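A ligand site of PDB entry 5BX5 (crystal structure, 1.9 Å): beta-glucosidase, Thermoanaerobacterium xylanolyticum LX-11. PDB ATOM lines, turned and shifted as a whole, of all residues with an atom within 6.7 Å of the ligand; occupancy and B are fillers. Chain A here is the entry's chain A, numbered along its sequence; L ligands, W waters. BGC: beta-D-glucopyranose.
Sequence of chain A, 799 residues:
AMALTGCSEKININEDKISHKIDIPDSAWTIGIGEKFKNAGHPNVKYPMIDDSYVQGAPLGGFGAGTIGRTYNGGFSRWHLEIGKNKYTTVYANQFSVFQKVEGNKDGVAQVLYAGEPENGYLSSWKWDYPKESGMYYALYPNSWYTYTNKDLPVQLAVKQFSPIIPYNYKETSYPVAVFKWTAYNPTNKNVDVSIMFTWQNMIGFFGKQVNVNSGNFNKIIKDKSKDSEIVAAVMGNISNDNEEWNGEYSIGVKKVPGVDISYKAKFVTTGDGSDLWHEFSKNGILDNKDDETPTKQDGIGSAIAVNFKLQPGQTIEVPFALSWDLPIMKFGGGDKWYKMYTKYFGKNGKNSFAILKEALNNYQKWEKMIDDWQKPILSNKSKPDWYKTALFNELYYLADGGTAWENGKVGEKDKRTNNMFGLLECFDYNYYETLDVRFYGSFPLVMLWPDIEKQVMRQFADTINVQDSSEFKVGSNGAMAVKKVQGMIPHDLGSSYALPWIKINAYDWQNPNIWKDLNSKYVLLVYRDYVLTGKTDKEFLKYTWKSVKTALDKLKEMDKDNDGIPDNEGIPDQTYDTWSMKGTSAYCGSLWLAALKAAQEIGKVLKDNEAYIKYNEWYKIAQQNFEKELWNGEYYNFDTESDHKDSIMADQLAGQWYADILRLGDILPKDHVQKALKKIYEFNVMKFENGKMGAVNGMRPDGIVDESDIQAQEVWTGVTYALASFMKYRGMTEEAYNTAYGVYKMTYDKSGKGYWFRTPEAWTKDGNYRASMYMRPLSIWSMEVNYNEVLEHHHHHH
The side-chain carboxylate (OE2) of Glu 762 lies within hydrogen-bond range of an oxygen (O6) of the ligand, 2.6 Å away.
The side-chain carboxylate of Asp 437 lies within hydrogen-bond range of an oxygen (O3) of the ligand (2.7 Å).
O4 of the ligand sits at hydrogen-bond distance from O of Thr 576 (2.7 Å).
The side-chain hydroxyl (OG1) of Thr 576 sits at hydrogen-bond distance from an oxygen (O4) of the ligand (2.8 Å).
O3 of the ligand sits at hydrogen-bond distance from NE2 of His 492.
The side-chain carboxylate (OE1) of Glu 426 sits at hydrogen-bond distance from an oxygen (O2) of the ligand (2.9 Å).
NH1 of Arg 771 is in hydrogen-bond range of O6 of the ligand.
NH2 of Arg 777 sits at hydrogen-bond distance from O4 of the ligand (2.9 Å).
The backbone NH (N) of Glu 762 lies within hydrogen-bond range of the backbone carbonyl oxygen (O) of Arg 771, at 3.3 Å.
The backbone carbonyl oxygen (O) of Ala 772 sits at hydrogen-bond distance from the backbone NH (N) of Glu 762.
OD2 of Asp 437 sits at hydrogen-bond distance from OG1 of Thr 576 (2.7 Å).
The side-chain hydroxyl (OH) of Tyr 775 is in hydrogen-bond range of the side-chain carboxylate (OE2) of Glu 426 (2.8 Å).
The backbone NH of Tyr 508 is in hydrogen-bond range of the side-chain carboxylate of Asp 493 (3.1 Å).
NE1 of Trp 717 sits at hydrogen-bond distance from OE1 of Glu 715, 2.9 Å away.
The indole nitrogen of Trp 510 is in hydrogen-bond range of the backbone carbonyl oxygen of Asp 578 (3.4 Å).
OE1 of Gln 712 lies within hydrogen-bond range of N of Thr 579 (3.0 Å).
Tyr 430 touches the ligand.
CD2 of Tyr 432 touches O2 of the ligand, at 3.8 Å.
Thr 435 touches the ligand (CG2 to O3, 3.9 Å).
CD1 of Tyr 508 touches O2 of the ligand, at 3.5 Å.
Trp 516 touches the ligand (CH2 to O3, 3.7 Å).
Asp 578 touches the ligand (OD1 to C6, 3.8 Å).
Gln 712 touches the ligand (NE2 to C6, 3.9 Å).
CH2 of Trp 717 touches C6 of the ligand, 3.5 Å away.
Tyr 775 touches the ligand (OH to C5, 3.6 Å).
Hydrophobic or aromatic side chains that line the ligand: Tyr 430, Tyr 432, His 492, Tyr 508, Trp 516 and Trp 717.
Of the 26 residues printed, 16 come within 4 Å of the ligand.
Along chain A the residues within 4 Å of the ligand span positions 426 to 777.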
ATOM      1  N   GLU A 426     -22.006  19.340 -14.000  1.00  0.00           N
ATOM      2  CA  GLU A 426     -22.347  18.028 -14.514  1.00  0.00           C
ATOM      3  C   GLU A 426     -21.815  16.950 -13.572  1.00  0.00           C
ATOM      4  O   GLU A 426     -22.487  15.961 -13.286  1.00  0.00           O
ATOM      5  CB  GLU A 426     -21.688  17.921 -15.881  1.00  0.00           C
ATOM      6  CG  GLU A 426     -21.819  16.610 -16.574  1.00  0.00           C
ATOM      7  CD  GLU A 426     -20.806  16.477 -17.708  1.00  0.00           C
ATOM      8  OE1 GLU A 426     -20.561  17.473 -18.424  1.00  0.00           O
ATOM      9  OE2 GLU A 426     -20.336  15.339 -17.922  1.00  0.00           O
ATOM     10  N   CYS A 427     -20.572  17.131 -13.136  1.00  0.00           N
ATOM     11  CA  CYS A 427     -19.898  16.287 -12.129  1.00  0.00           C
ATOM     12  C   CYS A 427     -18.530  16.890 -11.861  1.00  0.00           C
ATOM     13  O   CYS A 427     -18.225  17.968 -12.362  1.00  0.00           O
ATOM     14  CB  CYS A 427     -19.758  14.814 -12.549  1.00  0.00           C
ATOM     15  SG  CYS A 427     -18.615  14.509 -13.951  1.00  0.00           S
ATOM     16  N   TYR A 430     -15.662  15.703 -14.838  1.00  0.00           N
ATOM     17  CA  TYR A 430     -15.858  16.500 -16.030  1.00  0.00           C
ATOM     18  C   TYR A 430     -16.463  17.812 -15.555  1.00  0.00           C
ATOM     19  O   TYR A 430     -17.704  17.979 -15.490  1.00  0.00           O
ATOM     20  CB  TYR A 430     -16.792  15.790 -17.025  1.00  0.00           C
ATOM     21  CG  TYR A 430     -16.602  14.290 -17.196  1.00  0.00           C
ATOM     22  CD1 TYR A 430     -15.345  13.734 -17.366  1.00  0.00           C
ATOM     23  CD2 TYR A 430     -17.712  13.454 -17.256  1.00  0.00           C
ATOM     24  CE1 TYR A 430     -15.189  12.361 -17.558  1.00  0.00           C
ATOM     25  CE2 TYR A 430     -17.566  12.091 -17.451  1.00  0.00           C
ATOM     26  CZ  TYR A 430     -16.308  11.548 -17.618  1.00  0.00           C
ATOM     27  OH  TYR A 430     -16.201  10.196 -17.806  1.00  0.00           O
ATOM     28  N   TYR A 432     -17.716  20.857 -15.665  1.00  0.00           N
ATOM     29  CA  TYR A 432     -18.434  21.775 -16.551  1.00  0.00           C
ATOM     30  C   TYR A 432     -19.764  22.163 -15.908  1.00  0.00           C
ATOM     31  O   TYR A 432     -20.496  21.279 -15.426  1.00  0.00           O
ATOM     32  CB  TYR A 432     -18.749  21.099 -17.884  1.00  0.00           C
ATOM     33  CG  TYR A 432     -17.530  20.471 -18.526  1.00  0.00           C
ATOM     34  CD1 TYR A 432     -16.379  21.236 -18.699  1.00  0.00           C
ATOM     35  CD2 TYR A 432     -17.516  19.125 -18.901  1.00  0.00           C
ATOM     36  CE1 TYR A 432     -15.240  20.680 -19.246  1.00  0.00           C
ATOM     37  CE2 TYR A 432     -16.370  18.575 -19.451  1.00  0.00           C
ATOM     38  CZ  TYR A 432     -15.256  19.366 -19.614  1.00  0.00           C
ATOM     39  OH  TYR A 432     -14.111  18.856 -20.175  1.00  0.00           O
ATOM     40  N   THR A 435     -24.057  21.522 -18.055  1.00  0.00           N
ATOM     41  CA  THR A 435     -23.975  20.843 -19.321  1.00  0.00           C
ATOM     42  C   THR A 435     -25.382  20.560 -19.877  1.00  0.00           C
ATOM     43  O   THR A 435     -26.158  19.824 -19.274  1.00  0.00           O
ATOM     44  CB  THR A 435     -23.201  19.553 -19.193  1.00  0.00           C
ATOM     45  OG1 THR A 435     -21.891  19.864 -18.698  1.00  0.00           O
ATOM     46  CG2 THR A 435     -23.092  18.825 -20.521  1.00  0.00           C
ATOM     47  N   ASP A 437     -26.840  19.051 -22.492  1.00  0.00           N
ATOM     48  CA  ASP A 437     -27.306  17.746 -22.925  1.00  0.00           C
ATOM     49  C   ASP A 437     -27.597  16.813 -21.742  1.00  0.00           C
ATOM     50  O   ASP A 437     -28.371  15.853 -21.872  1.00  0.00           O
ATOM     51  CB  ASP A 437     -26.304  17.103 -23.902  1.00  0.00           C
ATOM     52  CG  ASP A 437     -24.893  17.137 -23.382  1.00  0.00           C
ATOM     53  OD1 ASP A 437     -24.299  18.234 -23.317  1.00  0.00           O
ATOM     54  OD2 ASP A 437     -24.360  16.072 -23.052  1.00  0.00           O
ATOM     55  N   VAL A 438     -26.963  17.113 -20.615  1.00  0.00           N
ATOM     56  CA  VAL A 438     -27.159  16.414 -19.333  1.00  0.00           C
ATOM     57  C   VAL A 438     -28.298  17.032 -18.509  1.00  0.00           C
ATOM     58  O   VAL A 438     -29.101  16.278 -17.906  1.00  0.00           O
ATOM     59  CB  VAL A 438     -25.865  16.456 -18.481  1.00  0.00           C
ATOM     60  CG1 VAL A 438     -26.076  15.796 -17.136  1.00  0.00           C
ATOM     61  CG2 VAL A 438     -24.731  15.746 -19.217  1.00  0.00           C
ATOM     62  N   HIS A 492     -22.396  23.656 -25.180  1.00  0.00           N
ATOM     63  CA  HIS A 492     -22.409  22.464 -24.340  1.00  0.00           C
ATOM     64  C   HIS A 492     -22.535  22.801 -22.862  1.00  0.00           C
ATOM     65  O   HIS A 492     -23.231  22.110 -22.123  1.00  0.00           O
ATOM     66  CB  HIS A 492     -21.109  21.695 -24.574  1.00  0.00           C
ATOM     67  CG  HIS A 492     -20.933  20.480 -23.727  1.00  0.00           C
ATOM     68  ND1 HIS A 492     -20.220  20.507 -22.544  1.00  0.00           N
ATOM     69  CD2 HIS A 492     -21.316  19.207 -23.902  1.00  0.00           C
ATOM     70  CE1 HIS A 492     -20.171  19.291 -22.027  1.00  0.00           C
ATOM     71  NE2 HIS A 492     -20.823  18.475 -22.840  1.00  0.00           N
ATOM     72  N   ASP A 493     -21.805  23.831 -22.431  1.00  0.00           N
ATOM     73  CA  ASP A 493     -21.735  24.208 -21.032  1.00  0.00           C
ATOM     74  C   ASP A 493     -21.416  25.678 -20.846  1.00  0.00           C
ATOM     75  O   ASP A 493     -21.080  26.393 -21.802  1.00  0.00           O
ATOM     76  CB  ASP A 493     -20.690  23.299 -20.344  1.00  0.00           C
ATOM     77  CG  ASP A 493     -19.286  23.521 -20.912  1.00  0.00           C
ATOM     78  OD1 ASP A 493     -18.690  24.576 -20.568  1.00  0.00           O
ATOM     79  OD2 ASP A 493     -18.821  22.632 -21.669  1.00  0.00           O
ATOM     80  N   TYR A 508     -15.871  22.274 -22.369  1.00  0.00           N
ATOM     81  CA  TYR A 508     -15.769  20.927 -22.899  1.00  0.00           C
ATOM     82  C   TYR A 508     -15.098  20.903 -24.285  1.00  0.00           C
ATOM     83  O   TYR A 508     -15.414  21.726 -25.150  1.00  0.00           O
ATOM     84  CB  TYR A 508     -17.176  20.347 -23.015  1.00  0.00           C
ATOM     85  CG  TYR A 508     -17.320  19.037 -23.738  1.00  0.00           C
ATOM     86  CD1 TYR A 508     -17.189  17.826 -23.074  1.00  0.00           C
ATOM     87  CD2 TYR A 508     -17.675  19.016 -25.091  1.00  0.00           C
ATOM     88  CE1 TYR A 508     -17.362  16.621 -23.752  1.00  0.00           C
ATOM     89  CE2 TYR A 508     -17.834  17.828 -25.761  1.00  0.00           C
ATOM     90  CZ  TYR A 508     -17.694  16.638 -25.096  1.00  0.00           C
ATOM     91  OH  TYR A 508     -17.899  15.466 -25.805  1.00  0.00           O
ATOM     92  N   TRP A 510     -13.780  17.431 -25.703  1.00  0.00           N
ATOM     93  CA  TRP A 510     -13.604  16.071 -26.228  1.00  0.00           C
ATOM     94  C   TRP A 510     -14.177  15.926 -27.630  1.00  0.00           C
ATOM     95  O   TRP A 510     -13.614  15.206 -28.490  1.00  0.00           O
ATOM     96  CB  TRP A 510     -14.238  15.042 -25.301  1.00  0.00           C
ATOM     97  CG  TRP A 510     -14.180  13.676 -25.844  1.00  0.00           C
ATOM     98  CD1 TRP A 510     -15.237  12.928 -26.299  1.00  0.00           C
ATOM     99  CD2 TRP A 510     -13.011  12.874 -26.007  1.00  0.00           C
ATOM    100  NE1 TRP A 510     -14.785  11.711 -26.732  1.00  0.00           N
ATOM    101  CE2 TRP A 510     -13.423  11.647 -26.556  1.00  0.00           C
ATOM    102  CE3 TRP A 510     -11.653  13.082 -25.736  1.00  0.00           C
ATOM    103  CZ2 TRP A 510     -12.536  10.624 -26.845  1.00  0.00           C
ATOM    104  CZ3 TRP A 510     -10.757  12.046 -26.036  1.00  0.00           C
ATOM    105  CH2 TRP A 510     -11.206  10.844 -26.576  1.00  0.00           C
ATOM    106  N   TRP A 516     -23.052  19.518 -32.635  1.00  0.00           N
ATOM    107  CA  TRP A 516     -23.965  18.534 -32.042  1.00  0.00           C
ATOM    108  C   TRP A 516     -25.389  18.687 -32.566  1.00  0.00           C
ATOM    109  O   TRP A 516     -25.836  19.788 -32.921  1.00  0.00           O
ATOM    110  CB  TRP A 516     -23.909  18.583 -30.512  1.00  0.00           C
ATOM    111  CG  TRP A 516     -22.717  17.877 -29.979  1.00  0.00           C
ATOM    112  CD1 TRP A 516     -21.549  17.590 -30.662  1.00  0.00           C
ATOM    113  CD2 TRP A 516     -22.522  17.364 -28.651  1.00  0.00           C
ATOM    114  NE1 TRP A 516     -20.670  16.916 -29.863  1.00  0.00           N
ATOM    115  CE2 TRP A 516     -21.242  16.764 -28.609  1.00  0.00           C
ATOM    116  CE3 TRP A 516     -23.320  17.326 -27.489  1.00  0.00           C
ATOM    117  CZ2 TRP A 516     -20.728  16.157 -27.469  1.00  0.00           C
ATOM    118  CZ3 TRP A 516     -22.809  16.701 -26.365  1.00  0.00           C
ATOM    119  CH2 TRP A 516     -21.529  16.150 -26.346  1.00  0.00           C
ATOM    120  N   GLN A 575     -23.451  14.210 -30.218  1.00  0.00           N
ATOM    121  CA  GLN A 575     -24.556  14.353 -29.258  1.00  0.00           C
ATOM    122  C   GLN A 575     -24.115  13.763 -27.917  1.00  0.00           C
ATOM    123  O   GLN A 575     -22.997  13.346 -27.771  1.00  0.00           O
ATOM    124  CB  GLN A 575     -25.851  13.715 -29.810  1.00  0.00           C
ATOM    125  CG  GLN A 575     -25.676  12.440 -30.612  1.00  0.00           C
ATOM    126  CD  GLN A 575     -25.064  11.307 -29.837  1.00  0.00           C
ATOM    127  OE1 GLN A 575     -25.475  11.006 -28.713  1.00  0.00           O
ATOM    128  NE2 GLN A 575     -24.134  10.609 -30.458  1.00  0.00           N
ATOM    129  N   THR A 576     -25.015  13.739 -26.945  1.00  0.00           N
ATOM    130  CA  THR A 576     -24.682  13.403 -25.555  1.00  0.00           C
ATOM    131  C   THR A 576     -23.951  12.085 -25.341  1.00  0.00           C
ATOM    132  O   THR A 576     -23.125  11.992 -24.449  1.00  0.00           O
ATOM    133  CB  THR A 576     -25.940  13.462 -24.640  1.00  0.00           C
ATOM    134  OG1 THR A 576     -25.533  13.640 -23.272  1.00  0.00           O
ATOM    135  CG2 THR A 576     -26.800  12.243 -24.795  1.00  0.00           C
ATOM    136  N   TYR A 577     -24.222  11.086 -26.186  1.00  0.00           N
ATOM    137  CA  TYR A 577     -23.473   9.847 -26.139  1.00  0.00           C
ATOM    138  C   TYR A 577     -22.179  10.116 -26.905  1.00  0.00           C
ATOM    139  O   TYR A 577     -22.019   9.703 -28.074  1.00  0.00           O
ATOM    140  CB  TYR A 577     -24.278   8.693 -26.748  1.00  0.00           C
ATOM    141  CG  TYR A 577     -25.584   8.420 -25.987  1.00  0.00           C
ATOM    142  CD1 TYR A 577     -26.749   9.109 -26.301  1.00  0.00           C
ATOM    143  CD2 TYR A 577     -25.634   7.493 -24.965  1.00  0.00           C
ATOM    144  CE1 TYR A 577     -27.941   8.871 -25.612  1.00  0.00           C
ATOM    145  CE2 TYR A 577     -26.823   7.239 -24.271  1.00  0.00           C
ATOM    146  CZ  TYR A 577     -27.957   7.939 -24.591  1.00  0.00           C
ATOM    147  OH  TYR A 577     -29.144   7.695 -23.907  1.00  0.00           O
ATOM    148  N   ASP A 578     -21.253  10.798 -26.235  1.00  0.00           N
ATOM    149  CA  ASP A 578     -20.144  11.432 -26.936  1.00  0.00           C
ATOM    150  C   ASP A 578     -18.983  10.513 -27.351  1.00  0.00           C
ATOM    151  O   ASP A 578     -17.950  11.013 -27.798  1.00  0.00           O
ATOM    152  CB  ASP A 578     -19.637  12.663 -26.172  1.00  0.00           C
ATOM    153  CG  ASP A 578     -18.882  12.328 -24.911  1.00  0.00           C
ATOM    154  OD1 ASP A 578     -18.957  11.181 -24.421  1.00  0.00           O
ATOM    155  OD2 ASP A 578     -18.240  13.253 -24.375  1.00  0.00           O
ATOM    156  N   THR A 579     -19.170   9.203 -27.233  1.00  0.00           N
ATOM    157  CA  THR A 579     -18.294   8.238 -27.931  1.00  0.00           C
ATOM    158  C   THR A 579     -19.083   7.257 -28.802  1.00  0.00           C
ATOM    159  O   THR A 579     -18.491   6.413 -29.456  1.00  0.00           O
ATOM    160  CB  THR A 579     -17.326   7.503 -26.986  1.00  0.00           C
ATOM    161  OG1 THR A 579     -18.021   6.867 -25.909  1.00  0.00           O
ATOM    162  CG2 THR A 579     -16.322   8.465 -26.408  1.00  0.00           C
ATOM    163  N   GLN A 712     -20.201   3.005 -24.473  1.00  0.00           N
ATOM    164  CA  GLN A 712     -21.440   3.659 -24.001  1.00  0.00           C
ATOM    165  C   GLN A 712     -22.666   2.801 -24.305  1.00  0.00           C
ATOM    166  O   GLN A 712     -23.633   2.806 -23.543  1.00  0.00           O
ATOM    167  CB  GLN A 712     -21.567   5.043 -24.622  1.00  0.00           C
ATOM    168  CG  GLN A 712     -20.564   6.035 -24.045  1.00  0.00           C
ATOM    169  CD  GLN A 712     -20.669   7.408 -24.635  1.00  0.00           C
ATOM    170  OE1 GLN A 712     -21.225   7.594 -25.732  1.00  0.00           O
ATOM    171  NE2 GLN A 712     -20.151   8.406 -23.919  1.00  0.00           N
ATOM    172  N   GLU A 715     -23.140   0.437 -21.403  1.00  0.00           N
ATOM    173  CA  GLU A 715     -23.346   1.066 -20.090  1.00  0.00           C
ATOM    174  C   GLU A 715     -24.845   1.214 -19.828  1.00  0.00           C
ATOM    175  O   GLU A 715     -25.639   1.411 -20.747  1.00  0.00           O
ATOM    176  CB  GLU A 715     -22.687   2.447 -20.028  1.00  0.00           C
ATOM    177  CG  GLU A 715     -21.162   2.451 -19.975  1.00  0.00           C
ATOM    178  CD  GLU A 715     -20.510   3.825 -19.911  1.00  0.00           C
ATOM    179  OE1 GLU A 715     -21.006   4.807 -20.552  1.00  0.00           O
ATOM    180  OE2 GLU A 715     -19.467   3.945 -19.234  1.00  0.00           O
ATOM    181  N   TRP A 717     -26.989   4.041 -18.113  1.00  0.00           N
ATOM    182  CA  TRP A 717     -26.879   5.415 -17.652  1.00  0.00           C
ATOM    183  C   TRP A 717     -28.012   5.638 -16.670  1.00  0.00           C
ATOM    184  O   TRP A 717     -29.194   5.452 -16.998  1.00  0.00           O
ATOM    185  CB  TRP A 717     -26.928   6.417 -18.807  1.00  0.00           C
ATOM    186  CG  TRP A 717     -25.630   6.518 -19.582  1.00  0.00           C
ATOM    187  CD1 TRP A 717     -24.577   5.641 -19.556  1.00  0.00           C
ATOM    188  CD2 TRP A 717     -25.277   7.542 -20.522  1.00  0.00           C
ATOM    189  NE1 TRP A 717     -23.593   6.055 -20.433  1.00  0.00           N
ATOM    190  CE2 TRP A 717     -24.004   7.215 -21.038  1.00  0.00           C
ATOM    191  CE3 TRP A 717     -25.911   8.701 -20.977  1.00  0.00           C
ATOM    192  CZ2 TRP A 717     -23.343   8.027 -21.967  1.00  0.00           C
ATOM    193  CZ3 TRP A 717     -25.268   9.507 -21.895  1.00  0.00           C
ATOM    194  CH2 TRP A 717     -23.972   9.169 -22.379  1.00  0.00           C
ATOM    195  N   GLU A 762     -22.800   8.619 -13.403  1.00  0.00           N
ATOM    196  CA  GLU A 762     -23.377   8.556 -14.749  1.00  0.00           C
ATOM    197  C   GLU A 762     -23.757   7.107 -15.115  1.00  0.00           C
ATOM    198  O   GLU A 762     -24.889   6.828 -15.484  1.00  0.00           O
ATOM    199  CB  GLU A 762     -22.369   9.090 -15.782  1.00  0.00           C
ATOM    200  CG  GLU A 762     -22.713   8.804 -17.233  1.00  0.00           C
ATOM    201  CD  GLU A 762     -23.633   9.837 -17.842  1.00  0.00           C
ATOM    202  OE1 GLU A 762     -24.828   9.918 -17.428  1.00  0.00           O
ATOM    203  OE2 GLU A 762     -23.151  10.575 -18.742  1.00  0.00           O
ATOM    204  N   ALA A 763     -22.793   6.207 -14.994  1.00  0.00           N
ATOM    205  CA  ALA A 763     -22.883   4.931 -15.680  1.00  0.00           C
ATOM    206  C   ALA A 763     -22.259   3.798 -14.914  1.00  0.00           C
ATOM    207  O   ALA A 763     -21.320   3.985 -14.138  1.00  0.00           O
ATOM    208  CB  ALA A 763     -22.205   5.030 -17.029  1.00  0.00           C
ATOM    209  N   ARG A 771     -18.563   4.812 -14.014  1.00  0.00           N
ATOM    210  CA  ARG A 771     -17.933   5.985 -14.607  1.00  0.00           C
ATOM    211  C   ARG A 771     -18.644   7.249 -14.109  1.00  0.00           C
ATOM    212  O   ARG A 771     -19.879   7.370 -14.230  1.00  0.00           O
ATOM    213  CB  ARG A 771     -17.972   5.924 -16.127  1.00  0.00           C
ATOM    214  CG  ARG A 771     -17.175   7.018 -16.804  1.00  0.00           C
ATOM    215  CD  ARG A 771     -17.035   6.778 -18.298  1.00  0.00           C
ATOM    216  NE  ARG A 771     -18.333   6.670 -18.989  1.00  0.00           N
ATOM    217  CZ  ARG A 771     -19.068   7.693 -19.417  1.00  0.00           C
ATOM    218  NH1 ARG A 771     -18.704   8.943 -19.197  1.00  0.00           N
ATOM    219  NH2 ARG A 771     -20.208   7.453 -20.050  1.00  0.00           N
ATOM    220  N   ALA A 772     -17.830   8.147 -13.541  1.00  0.00           N
ATOM    221  CA  ALA A 772     -18.168   9.506 -13.130  1.00  0.00           C
ATOM    222  C   ALA A 772     -19.165   9.544 -11.976  1.00  0.00           C
ATOM    223  O   ALA A 772     -20.357   9.780 -12.180  1.00  0.00           O
ATOM    224  CB  ALA A 772     -18.642  10.351 -14.309  1.00  0.00           C
ATOM    225  N   TYR A 775     -22.862  12.585 -10.156  1.00  0.00           N
ATOM    226  CA  TYR A 775     -23.275  13.003 -11.498  1.00  0.00           C
ATOM    227  C   TYR A 775     -24.672  13.633 -11.495  1.00  0.00           C
ATOM    228  O   TYR A 775     -25.551  13.206 -10.764  1.00  0.00           O
ATOM    229  CB  TYR A 775     -23.189  11.799 -12.456  1.00  0.00           C
ATOM    230  CG  TYR A 775     -22.980  12.223 -13.891  1.00  0.00           C
ATOM    231  CD1 TYR A 775     -21.715  12.634 -14.358  1.00  0.00           C
ATOM    232  CD2 TYR A 775     -24.029  12.262 -14.780  1.00  0.00           C
ATOM    233  CE1 TYR A 775     -21.544  13.081 -15.642  1.00  0.00           C
ATOM    234  CE2 TYR A 775     -23.869  12.718 -16.066  1.00  0.00           C
ATOM    235  CZ  TYR A 775     -22.618  13.110 -16.503  1.00  0.00           C
ATOM    236  OH  TYR A 775     -22.459  13.557 -17.779  1.00  0.00           O
ATOM    237  N   ARG A 777     -27.068  13.801 -14.026  1.00  0.00           N
ATOM    238  CA  ARG A 777     -28.130  13.170 -14.798  1.00  0.00           C
ATOM    239  C   ARG A 777     -29.182  12.383 -14.010  1.00  0.00           C
ATOM    240  O   ARG A 777     -30.370  12.512 -14.330  1.00  0.00           O
ATOM    241  CB  ARG A 777     -27.545  12.296 -15.932  1.00  0.00           C
ATOM    242  CG  ARG A 777     -28.360  12.393 -17.204  1.00  0.00           C
ATOM    243  CD  ARG A 777     -27.942  11.410 -18.292  1.00  0.00           C
ATOM    244  NE  ARG A 777     -26.560  11.619 -18.758  1.00  0.00           N
ATOM    245  CZ  ARG A 777     -26.170  12.289 -19.845  1.00  0.00           C
ATOM    246  NH1 ARG A 777     -27.019  12.892 -20.676  1.00  0.00           N
ATOM    247  NH2 ARG A 777     -24.853  12.337 -20.138  1.00  0.00           N
HETATM  248  C2  BGC L   1     -19.752  15.171 -21.400  1.00  0.00           C
HETATM  249  C3  BGC L   1     -21.252  14.985 -21.636  1.00  0.00           C
HETATM  250  C4  BGC L   1     -21.548  13.552 -22.006  1.00  0.00           C
HETATM  251  C5  BGC L   1     -20.995  12.594 -20.962  1.00  0.00           C
HETATM  252  C6  BGC L   1     -21.217  11.160 -21.374  1.00  0.00           C
HETATM  253  C1  BGC L   1     -19.261  14.120 -20.419  1.00  0.00           C
HETATM  254  O1  BGC L   1     -17.827  14.256 -20.369  1.00  0.00           O
HETATM  255  O2  BGC L   1     -19.462  16.446 -20.848  1.00  0.00           O
HETATM  256  O3  BGC L   1     -21.737  15.844 -22.648  1.00  0.00           O
HETATM  257  O4  BGC L   1     -22.972  13.379 -22.127  1.00  0.00           O
HETATM  258  O5  BGC L   1     -19.584  12.797 -20.835  1.00  0.00           O
HETATM  259  O6  BGC L   1     -21.043  10.300 -20.249  1.00  0.00           O
HETATM  260  O   HOH W   1     -15.432  15.451 -20.820  1.00  0.00           O
